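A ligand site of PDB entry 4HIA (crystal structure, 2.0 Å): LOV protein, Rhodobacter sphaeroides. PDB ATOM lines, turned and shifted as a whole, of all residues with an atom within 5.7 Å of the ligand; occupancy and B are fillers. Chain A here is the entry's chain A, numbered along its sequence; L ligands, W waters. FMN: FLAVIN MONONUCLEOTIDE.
The side-chain amide oxygen (OD1) of Asn 54 lies within hydrogen-bond range of an oxygen (O2') of the ligand (2.7 Å).
NH1 of Arg 72 is in salt-bridge range of O3P of the ligand, 2.8 Å away.
The guanidinium group of Arg 56 is in salt-bridge range of an oxygen (O2P) of the ligand (2.8 Å).
The side-chain amide nitrogen of Gln 59 lies within hydrogen-bond range of an oxygen (O2) of the ligand.
ND2 of Asn 87 lies within hydrogen-bond range of O2 of the ligand, at 2.9 Å.
NH2 of Arg 68 lies within salt-bridge range of O3P of the ligand (3.0 Å).
NE2 of Gln 118 lies within hydrogen-bond range of O4 of the ligand.
An oxygen (O4) of the ligand is in hydrogen-bond range of the side-chain amide nitrogen (ND2) of Asn 97, at 3.2 Å.
The side-chain sulfur (SG) of Cys 55 sits at hydrogen-bond distance from a nitrogen (N5) of the ligand (3.5 Å).
The side-chain amide oxygen of Asn 54 lies within hydrogen-bond range of the backbone NH of Arg 56, at 2.8 Å.
The backbone carbonyl oxygen (O) of Gln 30 is in hydrogen-bond range of the side-chain amide nitrogen (ND2) of Asn 54 (3.4 Å).
The side-chain amide oxygen (OE1) of Gln 59 is in hydrogen-bond range of the side-chain amide nitrogen (ND2) of Asn 64 (3.3 Å).
The side-chain amide nitrogen (ND2) of Asn 97 sits at hydrogen-bond distance from the side-chain amide oxygen (OD1) of Asn 87 (2.8 Å).
The side-chain amide nitrogen (NE2) of Gln 118 sits at hydrogen-bond distance from the side-chain hydroxyl (OG1) of Thr 21, 3.3 Å away.
The side-chain amide oxygen (OD1) of Asn 97 lies within hydrogen-bond range of the backbone NH (N) of Leu 99, at 3.5 Å.
N of Val 23 is in hydrogen-bond range of O of Phe 114 (2.8 Å).
O of Gly 116 sits at hydrogen-bond distance from N of Thr 21.
Thr 21 touches the ligand.
Val 23 touches the ligand (CG2 to C7M, 3.7 Å).
CD1 of Leu 58 touches O4 of the ligand, 3.5 Å away.
Ile 71 touches the ligand (CG2 to O3', 3.6 Å).
Leu 75 touches the ligand.
Leu 85 touches the ligand.
Leu 99 touches the ligand (CD1 to N5, 3.6 Å).
Leu 101 touches the ligand (CD2 to C7, 3.5 Å).
Phe 114 touches the ligand (O to C7M, 3.3 Å).
Leu 115 touches the ligand (C to C7M, 3.6 Å).
N of Gly 116 touches C7M of the ligand (3.5 Å).
Hydrophobic or aromatic side chains that line the ligand: Val 23, Leu 58, Ile 71, Leu 75, Leu 85, Leu 99, Leu 101 and Phe 114.
Of the 27 residues printed, 20 come within 4 Å of the ligand.
Water W3 lies within hydrogen-bond range of O3' of the ligand (2.7 Å), OE1 of Gln 30 (2.9 Å) and ND2 of Asn 54 (2.9 Å).
Water W1 lies within hydrogen-bond range of the backbone NH of Cys 55 (2.8 Å), the backbone carbonyl oxygen of Gln 30 (3.0 Å), an oxygen (O2') of the ligand (3.0 Å) and the side-chain amide nitrogen of Asn 54 (3.5 Å).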
ATOM      1  N   THR A  21     -29.995  28.578 -20.984  1.00  0.00           N
ATOM      2  CA  THR A  21     -28.609  28.115 -21.117  1.00  0.00           C
ATOM      3  C   THR A  21     -28.527  27.275 -22.383  1.00  0.00           C
ATOM      4  O   THR A  21     -29.504  26.648 -22.780  1.00  0.00           O
ATOM      5  CB  THR A  21     -28.173  27.272 -19.928  1.00  0.00           C
ATOM      6  OG1 THR A  21     -29.165  26.271 -19.670  1.00  0.00           O
ATOM      7  CG2 THR A  21     -28.002  28.134 -18.677  1.00  0.00           C
ATOM      8  N   LEU A  22     -27.349  27.250 -23.004  1.00  0.00           N
ATOM      9  CA  LEU A  22     -27.128  26.381 -24.150  1.00  0.00           C
ATOM     10  C   LEU A  22     -25.874  25.530 -23.913  1.00  0.00           C
ATOM     11  O   LEU A  22     -24.852  26.044 -23.461  1.00  0.00           O
ATOM     12  CB  LEU A  22     -26.950  27.201 -25.435  1.00  0.00           C
ATOM     13  CG  LEU A  22     -27.153  26.386 -26.716  1.00  0.00           C
ATOM     14  CD1 LEU A  22     -28.627  26.044 -26.876  1.00  0.00           C
ATOM     15  CD2 LEU A  22     -26.631  27.135 -27.942  1.00  0.00           C
ATOM     16  N   VAL A  23     -25.974  24.236 -24.205  1.00  0.00           N
ATOM     17  CA  VAL A  23     -24.844  23.332 -24.006  1.00  0.00           C
ATOM     18  C   VAL A  23     -24.484  22.643 -25.314  1.00  0.00           C
ATOM     19  O   VAL A  23     -25.366  22.164 -26.033  1.00  0.00           O
ATOM     20  CB  VAL A  23     -25.177  22.262 -22.928  1.00  0.00           C
ATOM     21  CG1 VAL A  23     -24.220  21.084 -23.024  1.00  0.00           C
ATOM     22  CG2 VAL A  23     -25.133  22.857 -21.532  1.00  0.00           C
ATOM     23  N   MET A  25     -23.397  19.622 -27.270  1.00  0.00           N
ATOM     24  CA  MET A  25     -23.429  18.190 -27.038  1.00  0.00           C
ATOM     25  C   MET A  25     -22.286  17.473 -27.751  1.00  0.00           C
ATOM     26  O   MET A  25     -22.039  16.286 -27.506  1.00  0.00           O
ATOM     27  CB  MET A  25     -24.783  17.611 -27.478  1.00  0.00           C
ATOM     28  CG  MET A  25     -25.977  18.158 -26.711  1.00  0.00           C
ATOM     29  SD  MET A  25     -25.879  17.801 -24.956  1.00  0.00           S
ATOM     30  CE  MET A  25     -26.306  16.053 -24.996  1.00  0.00           C
ATOM     31  N   GLN A  30     -19.890  18.248 -22.072  1.00  0.00           N
ATOM     32  CA  GLN A  30     -21.167  18.948 -22.230  1.00  0.00           C
ATOM     33  C   GLN A  30     -21.170  20.290 -21.495  1.00  0.00           C
ATOM     34  O   GLN A  30     -21.931  20.482 -20.547  1.00  0.00           O
ATOM     35  CB  GLN A  30     -22.339  18.051 -21.811  1.00  0.00           C
ATOM     36  CG  GLN A  30     -22.425  16.750 -22.671  1.00  0.00           C
ATOM     37  CD  GLN A  30     -23.509  15.768 -22.241  1.00  0.00           C
ATOM     38  OE1 GLN A  30     -24.104  15.915 -21.172  1.00  0.00           O
ATOM     39  NE2 GLN A  30     -23.758  14.760 -23.069  1.00  0.00           N
ATOM     40  N   PHE A  39     -30.488  33.938 -16.026  1.00  0.00           N
ATOM     41  CA  PHE A  39     -29.874  32.762 -15.420  1.00  0.00           C
ATOM     42  C   PHE A  39     -28.774  33.206 -14.439  1.00  0.00           C
ATOM     43  O   PHE A  39     -28.680  32.680 -13.331  1.00  0.00           O
ATOM     44  CB  PHE A  39     -29.290  31.822 -16.491  1.00  0.00           C
ATOM     45  CG  PHE A  39     -28.501  30.644 -15.913  1.00  0.00           C
ATOM     46  CD1 PHE A  39     -29.137  29.481 -15.534  1.00  0.00           C
ATOM     47  CD2 PHE A  39     -27.123  30.728 -15.780  1.00  0.00           C
ATOM     48  CE1 PHE A  39     -28.421  28.407 -15.030  1.00  0.00           C
ATOM     49  CE2 PHE A  39     -26.397  29.673 -15.268  1.00  0.00           C
ATOM     50  CZ  PHE A  39     -27.046  28.513 -14.893  1.00  0.00           C
ATOM     51  N   ASN A  54     -19.775  22.214 -17.190  1.00  0.00           N
ATOM     52  CA  ASN A  54     -21.046  21.502 -17.150  1.00  0.00           C
ATOM     53  C   ASN A  54     -21.952  22.156 -16.085  1.00  0.00           C
ATOM     54  O   ASN A  54     -21.469  22.562 -15.024  1.00  0.00           O
ATOM     55  CB  ASN A  54     -20.813  20.018 -16.829  1.00  0.00           C
ATOM     56  CG  ASN A  54     -22.103  19.204 -16.868  1.00  0.00           C
ATOM     57  OD1 ASN A  54     -22.944  19.307 -15.981  1.00  0.00           O
ATOM     58  ND2 ASN A  54     -22.245  18.354 -17.895  1.00  0.00           N
ATOM     59  N   CYS A  55     -23.246  22.231 -16.364  1.00  0.00           N
ATOM     60  CA  CYS A  55     -24.183  22.922 -15.471  1.00  0.00           C
ATOM     61  C   CYS A  55     -24.416  22.236 -14.112  1.00  0.00           C
ATOM     62  O   CYS A  55     -25.082  22.798 -13.245  1.00  0.00           O
ATOM     63  CB  CYS A  55     -25.519  23.162 -16.190  1.00  0.00           C
ATOM     64  SG  CYS A  55     -26.263  24.754 -15.759  1.00  0.00           S
ATOM     65  N   ARG A  56     -23.841  21.050 -13.925  1.00  0.00           N
ATOM     66  CA  ARG A  56     -24.008  20.325 -12.671  1.00  0.00           C
ATOM     67  C   ARG A  56     -23.357  21.035 -11.481  1.00  0.00           C
ATOM     68  O   ARG A  56     -23.522  20.607 -10.337  1.00  0.00           O
ATOM     69  CB  ARG A  56     -23.460  18.896 -12.781  1.00  0.00           C
ATOM     70  CG  ARG A  56     -21.932  18.808 -12.814  1.00  0.00           C
ATOM     71  CD  ARG A  56     -21.474  17.369 -12.678  1.00  0.00           C
ATOM     72  NE  ARG A  56     -21.980  16.506 -13.747  1.00  0.00           N
ATOM     73  CZ  ARG A  56     -21.373  16.363 -14.927  1.00  0.00           C
ATOM     74  NH1 ARG A  56     -20.253  17.030 -15.188  1.00  0.00           N
ATOM     75  NH2 ARG A  56     -21.886  15.553 -15.845  1.00  0.00           N
ATOM     76  N   LEU A  58     -24.294  23.599 -10.225  1.00  0.00           N
ATOM     77  CA  LEU A  58     -25.407  24.087  -9.397  1.00  0.00           C
ATOM     78  C   LEU A  58     -25.857  23.071  -8.336  1.00  0.00           C
ATOM     79  O   LEU A  58     -26.677  23.384  -7.471  1.00  0.00           O
ATOM     80  CB  LEU A  58     -26.594  24.465 -10.272  1.00  0.00           C
ATOM     81  CG  LEU A  58     -26.385  25.677 -11.194  1.00  0.00           C
ATOM     82  CD1 LEU A  58     -27.608  25.895 -12.030  1.00  0.00           C
ATOM     83  CD2 LEU A  58     -26.098  26.937 -10.379  1.00  0.00           C
ATOM     84  N   GLN A  59     -25.316  21.852  -8.397  1.00  0.00           N
ATOM     85  CA  GLN A  59     -25.729  20.817  -7.451  1.00  0.00           C
ATOM     86  C   GLN A  59     -24.646  20.557  -6.407  1.00  0.00           C
ATOM     87  O   GLN A  59     -23.506  20.997  -6.573  1.00  0.00           O
ATOM     88  CB  GLN A  59     -26.032  19.522  -8.216  1.00  0.00           C
ATOM     89  CG  GLN A  59     -27.076  19.693  -9.293  1.00  0.00           C
ATOM     90  CD  GLN A  59     -27.328  18.419 -10.056  1.00  0.00           C
ATOM     91  OE1 GLN A  59     -27.430  17.336  -9.464  1.00  0.00           O
ATOM     92  NE2 GLN A  59     -27.422  18.512 -11.384  1.00  0.00           N
ATOM     93  N   ASN A  64     -30.183  14.628  -6.093  1.00  0.00           N
ATOM     94  CA  ASN A  64     -30.936  14.517  -7.346  1.00  0.00           C
ATOM     95  C   ASN A  64     -30.581  13.278  -8.131  1.00  0.00           C
ATOM     96  O   ASN A  64     -30.521  13.343  -9.360  1.00  0.00           O
ATOM     97  CB  ASN A  64     -30.744  15.757  -8.237  1.00  0.00           C
ATOM     98  CG  ASN A  64     -30.970  17.041  -7.490  1.00  0.00           C
ATOM     99  OD1 ASN A  64     -32.064  17.301  -7.000  1.00  0.00           O
ATOM    100  ND2 ASN A  64     -29.927  17.869  -7.402  1.00  0.00           N
ATOM    101  N   ARG A  68     -31.207  13.176 -12.177  1.00  0.00           N
ATOM    102  CA  ARG A  68     -30.010  13.181 -13.016  1.00  0.00           C
ATOM    103  C   ARG A  68     -29.996  11.980 -13.953  1.00  0.00           C
ATOM    104  O   ARG A  68     -29.559  12.084 -15.089  1.00  0.00           O
ATOM    105  CB  ARG A  68     -28.732  13.209 -12.152  1.00  0.00           C
ATOM    106  CG  ARG A  68     -28.393  14.601 -11.580  1.00  0.00           C
ATOM    107  CD  ARG A  68     -27.064  14.631 -10.809  1.00  0.00           C
ATOM    108  NE  ARG A  68     -27.146  13.831  -9.576  1.00  0.00           N
ATOM    109  CZ  ARG A  68     -26.574  12.646  -9.426  1.00  0.00           C
ATOM    110  NH1 ARG A  68     -26.696  11.980  -8.276  1.00  0.00           N
ATOM    111  NH2 ARG A  68     -25.845  12.140 -10.410  1.00  0.00           N
ATOM    112  N   ALA A  69     -30.463  10.830 -13.467  1.00  0.00           N
ATOM    113  CA  ALA A  69     -30.587   9.653 -14.325  1.00  0.00           C
ATOM    114  C   ALA A  69     -31.596   9.926 -15.427  1.00  0.00           C
ATOM    115  O   ALA A  69     -31.381   9.547 -16.592  1.00  0.00           O
ATOM    116  CB  ALA A  69     -30.978   8.422 -13.520  1.00  0.00           C
ATOM    117  N   ILE A  71     -32.345  12.891 -16.604  1.00  0.00           N
ATOM    118  CA  ILE A  71     -31.667  13.859 -17.473  1.00  0.00           C
ATOM    119  C   ILE A  71     -30.689  13.180 -18.420  1.00  0.00           C
ATOM    120  O   ILE A  71     -30.679  13.472 -19.620  1.00  0.00           O
ATOM    121  CB  ILE A  71     -30.948  14.944 -16.629  1.00  0.00           C
ATOM    122  CG1 ILE A  71     -31.966  15.914 -16.043  1.00  0.00           C
ATOM    123  CG2 ILE A  71     -29.952  15.710 -17.494  1.00  0.00           C
ATOM    124  CD1 ILE A  71     -31.424  16.741 -14.871  1.00  0.00           C
ATOM    125  N   ARG A  72     -29.856  12.275 -17.885  1.00  0.00           N
ATOM    126  CA  ARG A  72     -28.894  11.581 -18.740  1.00  0.00           C
ATOM    127  C   ARG A  72     -29.608  10.804 -19.849  1.00  0.00           C
ATOM    128  O   ARG A  72     -29.147  10.789 -20.991  1.00  0.00           O
ATOM    129  CB  ARG A  72     -27.953  10.672 -17.928  1.00  0.00           C
ATOM    130  CG  ARG A  72     -27.009  11.432 -16.969  1.00  0.00           C
ATOM    131  CD  ARG A  72     -25.880  10.533 -16.429  1.00  0.00           C
ATOM    132  NE  ARG A  72     -26.406   9.356 -15.742  1.00  0.00           N
ATOM    133  CZ  ARG A  72     -26.773   9.332 -14.463  1.00  0.00           C
ATOM    134  NH1 ARG A  72     -26.674  10.430 -13.718  1.00  0.00           N
ATOM    135  NH2 ARG A  72     -27.243   8.216 -13.938  1.00  0.00           N
ATOM    136  N   LEU A  75     -30.973  13.327 -22.513  1.00  0.00           N
ATOM    137  CA  LEU A  75     -29.844  13.861 -23.281  1.00  0.00           C
ATOM    138  C   LEU A  75     -29.372  12.851 -24.315  1.00  0.00           C
ATOM    139  O   LEU A  75     -29.127  13.196 -25.468  1.00  0.00           O
ATOM    140  CB  LEU A  75     -28.688  14.182 -22.339  1.00  0.00           C
ATOM    141  CG  LEU A  75     -28.413  15.641 -21.981  1.00  0.00           C
ATOM    142  CD1 LEU A  75     -29.630  16.528 -22.131  1.00  0.00           C
ATOM    143  CD2 LEU A  75     -27.852  15.742 -20.578  1.00  0.00           C
ATOM    144  N   LEU A  85     -35.051  19.995  -9.830  1.00  0.00           N
ATOM    145  CA  LEU A  85     -33.727  19.753  -9.229  1.00  0.00           C
ATOM    146  C   LEU A  85     -33.510  20.637  -8.013  1.00  0.00           C
ATOM    147  O   LEU A  85     -33.860  21.815  -8.046  1.00  0.00           O
ATOM    148  CB  LEU A  85     -32.623  20.104 -10.224  1.00  0.00           C
ATOM    149  CG  LEU A  85     -32.590  19.264 -11.504  1.00  0.00           C
ATOM    150  CD1 LEU A  85     -31.578  19.823 -12.474  1.00  0.00           C
ATOM    151  CD2 LEU A  85     -32.253  17.821 -11.143  1.00  0.00           C
ATOM    152  N   ARG A  86     -32.906  20.088  -6.958  1.00  0.00           N
ATOM    153  CA  ARG A  86     -32.325  20.932  -5.903  1.00  0.00           C
ATOM    154  C   ARG A  86     -31.000  21.524  -6.385  1.00  0.00           C
ATOM    155  O   ARG A  86     -30.031  20.794  -6.702  1.00  0.00           O
ATOM    156  CB  ARG A  86     -32.158  20.119  -4.599  1.00  0.00           C
ATOM    157  CG  ARG A  86     -31.421  20.834  -3.439  1.00  0.00           C
ATOM    158  CD  ARG A  86     -32.018  22.197  -3.040  1.00  0.00           C
ATOM    159  NE  ARG A  86     -33.464  22.221  -2.747  1.00  0.00           N
ATOM    160  CZ  ARG A  86     -34.001  22.262  -1.531  1.00  0.00           C
ATOM    161  NH1 ARG A  86     -33.230  22.263  -0.437  1.00  0.00           N
ATOM    162  NH2 ARG A  86     -35.326  22.323  -1.386  1.00  0.00           N
ATOM    163  N   ASN A  87     -30.960  22.853  -6.453  1.00  0.00           N
ATOM    164  CA  ASN A  87     -29.783  23.611  -6.882  1.00  0.00           C
ATOM    165  C   ASN A  87     -29.399  24.613  -5.793  1.00  0.00           C
ATOM    166  O   ASN A  87     -30.154  24.836  -4.839  1.00  0.00           O
ATOM    167  CB  ASN A  87     -30.073  24.383  -8.189  1.00  0.00           C
ATOM    168  CG  ASN A  87     -29.943  23.527  -9.451  1.00  0.00           C
ATOM    169  OD1 ASN A  87     -30.173  24.023 -10.560  1.00  0.00           O
ATOM    170  ND2 ASN A  87     -29.597  22.254  -9.283  1.00  0.00           N
ATOM    171  N   ASN A  97     -35.470  24.062  -8.749  1.00  0.00           N
ATOM    172  CA  ASN A  97     -35.328  24.484 -10.128  1.00  0.00           C
ATOM    173  C   ASN A  97     -36.186  23.556 -10.958  1.00  0.00           C
ATOM    174  O   ASN A  97     -35.953  22.350 -10.963  1.00  0.00           O
ATOM    175  CB  ASN A  97     -33.838  24.351 -10.512  1.00  0.00           C
ATOM    176  CG  ASN A  97     -33.545  24.650 -11.968  1.00  0.00           C
ATOM    177  OD1 ASN A  97     -34.449  24.898 -12.781  1.00  0.00           O
ATOM    178  ND2 ASN A  97     -32.267  24.648 -12.316  1.00  0.00           N
ATOM    179  N   LEU A  99     -36.488  22.550 -14.312  1.00  0.00           N
ATOM    180  CA  LEU A  99     -35.639  22.624 -15.505  1.00  0.00           C
ATOM    181  C   LEU A  99     -36.360  22.088 -16.746  1.00  0.00           C
ATOM    182  O   LEU A  99     -36.881  20.955 -16.733  1.00  0.00           O
ATOM    183  CB  LEU A  99     -34.352  21.827 -15.260  1.00  0.00           C
ATOM    184  CG  LEU A  99     -33.373  21.688 -16.437  1.00  0.00           C
ATOM    185  CD1 LEU A  99     -32.788  23.038 -16.814  1.00  0.00           C
ATOM    186  CD2 LEU A  99     -32.246  20.718 -16.055  1.00  0.00           C
ATOM    187  N   LEU A 101     -35.615  20.997 -20.557  1.00  0.00           N
ATOM    188  CA  LEU A 101     -34.545  20.653 -21.500  1.00  0.00           C
ATOM    189  C   LEU A 101     -35.130  20.466 -22.900  1.00  0.00           C
ATOM    190  O   LEU A 101     -36.162  19.808 -23.059  1.00  0.00           O
ATOM    191  CB  LEU A 101     -33.825  19.344 -21.062  1.00  0.00           C
ATOM    192  CG  LEU A 101     -32.908  19.488 -19.849  1.00  0.00           C
ATOM    193  CD1 LEU A 101     -32.498  18.130 -19.250  1.00  0.00           C
ATOM    194  CD2 LEU A 101     -31.657  20.293 -20.229  1.00  0.00           C
ATOM    195  N   PHE A 114     -28.125  21.281 -26.604  1.00  0.00           N
ATOM    196  CA  PHE A 114     -29.325  21.214 -25.781  1.00  0.00           C
ATOM    197  C   PHE A 114     -29.522  22.589 -25.131  1.00  0.00           C
ATOM    198  O   PHE A 114     -28.548  23.247 -24.724  1.00  0.00           O
ATOM    199  CB  PHE A 114     -29.193  20.129 -24.696  1.00  0.00           C
ATOM    200  CG  PHE A 114     -30.138  18.975 -24.886  1.00  0.00           C
ATOM    201  CD1 PHE A 114     -31.417  19.010 -24.324  1.00  0.00           C
ATOM    202  CD2 PHE A 114     -29.754  17.854 -25.615  1.00  0.00           C
ATOM    203  CE1 PHE A 114     -32.298  17.949 -24.494  1.00  0.00           C
ATOM    204  CE2 PHE A 114     -30.637  16.764 -25.777  1.00  0.00           C
ATOM    205  CZ  PHE A 114     -31.911  16.823 -25.215  1.00  0.00           C
ATOM    206  N   LEU A 115     -30.787  23.024 -25.070  1.00  0.00           N
ATOM    207  CA  LEU A 115     -31.162  24.275 -24.387  1.00  0.00           C
ATOM    208  C   LEU A 115     -31.753  23.913 -23.030  1.00  0.00           C
ATOM    209  O   LEU A 115     -32.495  22.925 -22.912  1.00  0.00           O
ATOM    210  CB  LEU A 115     -32.185  25.071 -25.224  1.00  0.00           C
ATOM    211  CG  LEU A 115     -32.779  26.374 -24.653  1.00  0.00           C
ATOM    212  CD1 LEU A 115     -33.095  27.376 -25.779  1.00  0.00           C
ATOM    213  CD2 LEU A 115     -34.052  26.140 -23.831  1.00  0.00           C
ATOM    214  N   GLY A 116     -31.431  24.693 -22.002  1.00  0.00           N
ATOM    215  CA  GLY A 116     -32.021  24.480 -20.700  1.00  0.00           C
ATOM    216  C   GLY A 116     -32.617  25.786 -20.220  1.00  0.00           C
ATOM    217  O   GLY A 116     -32.009  26.834 -20.397  1.00  0.00           O
ATOM    218  N   GLN A 118     -34.565  27.552 -16.816  1.00  0.00           N
ATOM    219  CA  GLN A 118     -34.765  27.297 -15.378  1.00  0.00           C
ATOM    220  C   GLN A 118     -35.864  28.175 -14.774  1.00  0.00           C
ATOM    221  O   GLN A 118     -35.785  29.406 -14.826  1.00  0.00           O
ATOM    222  CB  GLN A 118     -33.445  27.545 -14.620  1.00  0.00           C
ATOM    223  CG  GLN A 118     -32.302  26.615 -15.029  1.00  0.00           C
ATOM    224  CD  GLN A 118     -31.598  27.022 -16.320  1.00  0.00           C
ATOM    225  OE1 GLN A 118     -31.833  28.116 -16.869  1.00  0.00           O
ATOM    226  NE2 GLN A 118     -30.706  26.156 -16.803  1.00  0.00           N
HETATM  227  N1  FMN L   1     -28.354  20.743 -13.888  1.00  0.00           N
HETATM  228  C2  FMN L   1     -28.688  21.524 -12.800  1.00  0.00           C
HETATM  229  O2  FMN L   1     -28.555  21.056 -11.671  1.00  0.00           O
HETATM  230  N3  FMN L   1     -29.187  22.792 -12.969  1.00  0.00           N
HETATM  231  C4  FMN L   1     -29.355  23.306 -14.247  1.00  0.00           C
HETATM  232  O4  FMN L   1     -29.808  24.441 -14.404  1.00  0.00           O
HETATM  233  C4A FMN L   1     -29.007  22.535 -15.351  1.00  0.00           C
HETATM  234  N5  FMN L   1     -29.158  23.040 -16.618  1.00  0.00           N
HETATM  235  C5A FMN L   1     -28.811  22.256 -17.703  1.00  0.00           C
HETATM  236  C6  FMN L   1     -28.960  22.774 -18.988  1.00  0.00           C
HETATM  237  C7  FMN L   1     -28.618  21.988 -20.086  1.00  0.00           C
HETATM  238  C7M FMN L   1     -28.782  22.541 -21.473  1.00  0.00           C
HETATM  239  C8  FMN L   1     -28.116  20.701 -19.891  1.00  0.00           C
HETATM  240  C8M FMN L   1     -27.753  19.857 -21.082  1.00  0.00           C
HETATM  241  C9  FMN L   1     -27.966  20.183 -18.605  1.00  0.00           C
HETATM  242  C9A FMN L   1     -28.318  20.968 -17.504  1.00  0.00           C
HETATM  243  N10 FMN L   1     -28.144  20.478 -16.225  1.00  0.00           N
HETATM  244  C10 FMN L   1     -28.509  21.254 -15.163  1.00  0.00           C
HETATM  245  C1' FMN L   1     -27.683  19.057 -15.957  1.00  0.00           C
HETATM  246  C2' FMN L   1     -26.251  18.720 -15.699  1.00  0.00           C
HETATM  247  O2' FMN L   1     -25.520  19.449 -16.649  1.00  0.00           O
HETATM  248  C3' FMN L   1     -26.079  17.205 -15.869  1.00  0.00           C
HETATM  249  O3' FMN L   1     -26.516  16.827 -17.164  1.00  0.00           O
HETATM  250  C4' FMN L   1     -26.898  16.378 -14.861  1.00  0.00           C
HETATM  251  O4' FMN L   1     -26.487  16.644 -13.526  1.00  0.00           O
HETATM  252  C5' FMN L   1     -26.841  14.864 -15.129  1.00  0.00           C
HETATM  253  O5' FMN L   1     -25.497  14.434 -15.324  1.00  0.00           O
HETATM  254  P   FMN L   1     -24.613  13.899 -14.101  1.00  0.00           P
HETATM  255  O1P FMN L   1     -23.344  13.368 -14.721  1.00  0.00           O
HETATM  256  O2P FMN L   1     -24.314  15.083 -13.212  1.00  0.00           O
HETATM  257  O3P FMN L   1     -25.322  12.824 -13.320  1.00  0.00           O
HETATM  258  O   HOH W   1     -24.188  21.146 -18.723  1.00  0.00           O
HETATM  259  O   HOH W   2     -20.918  12.610 -13.514  1.00  0.00           O
HETATM  260  O   HOH W   3     -24.870  17.811 -19.116  1.00  0.00           O
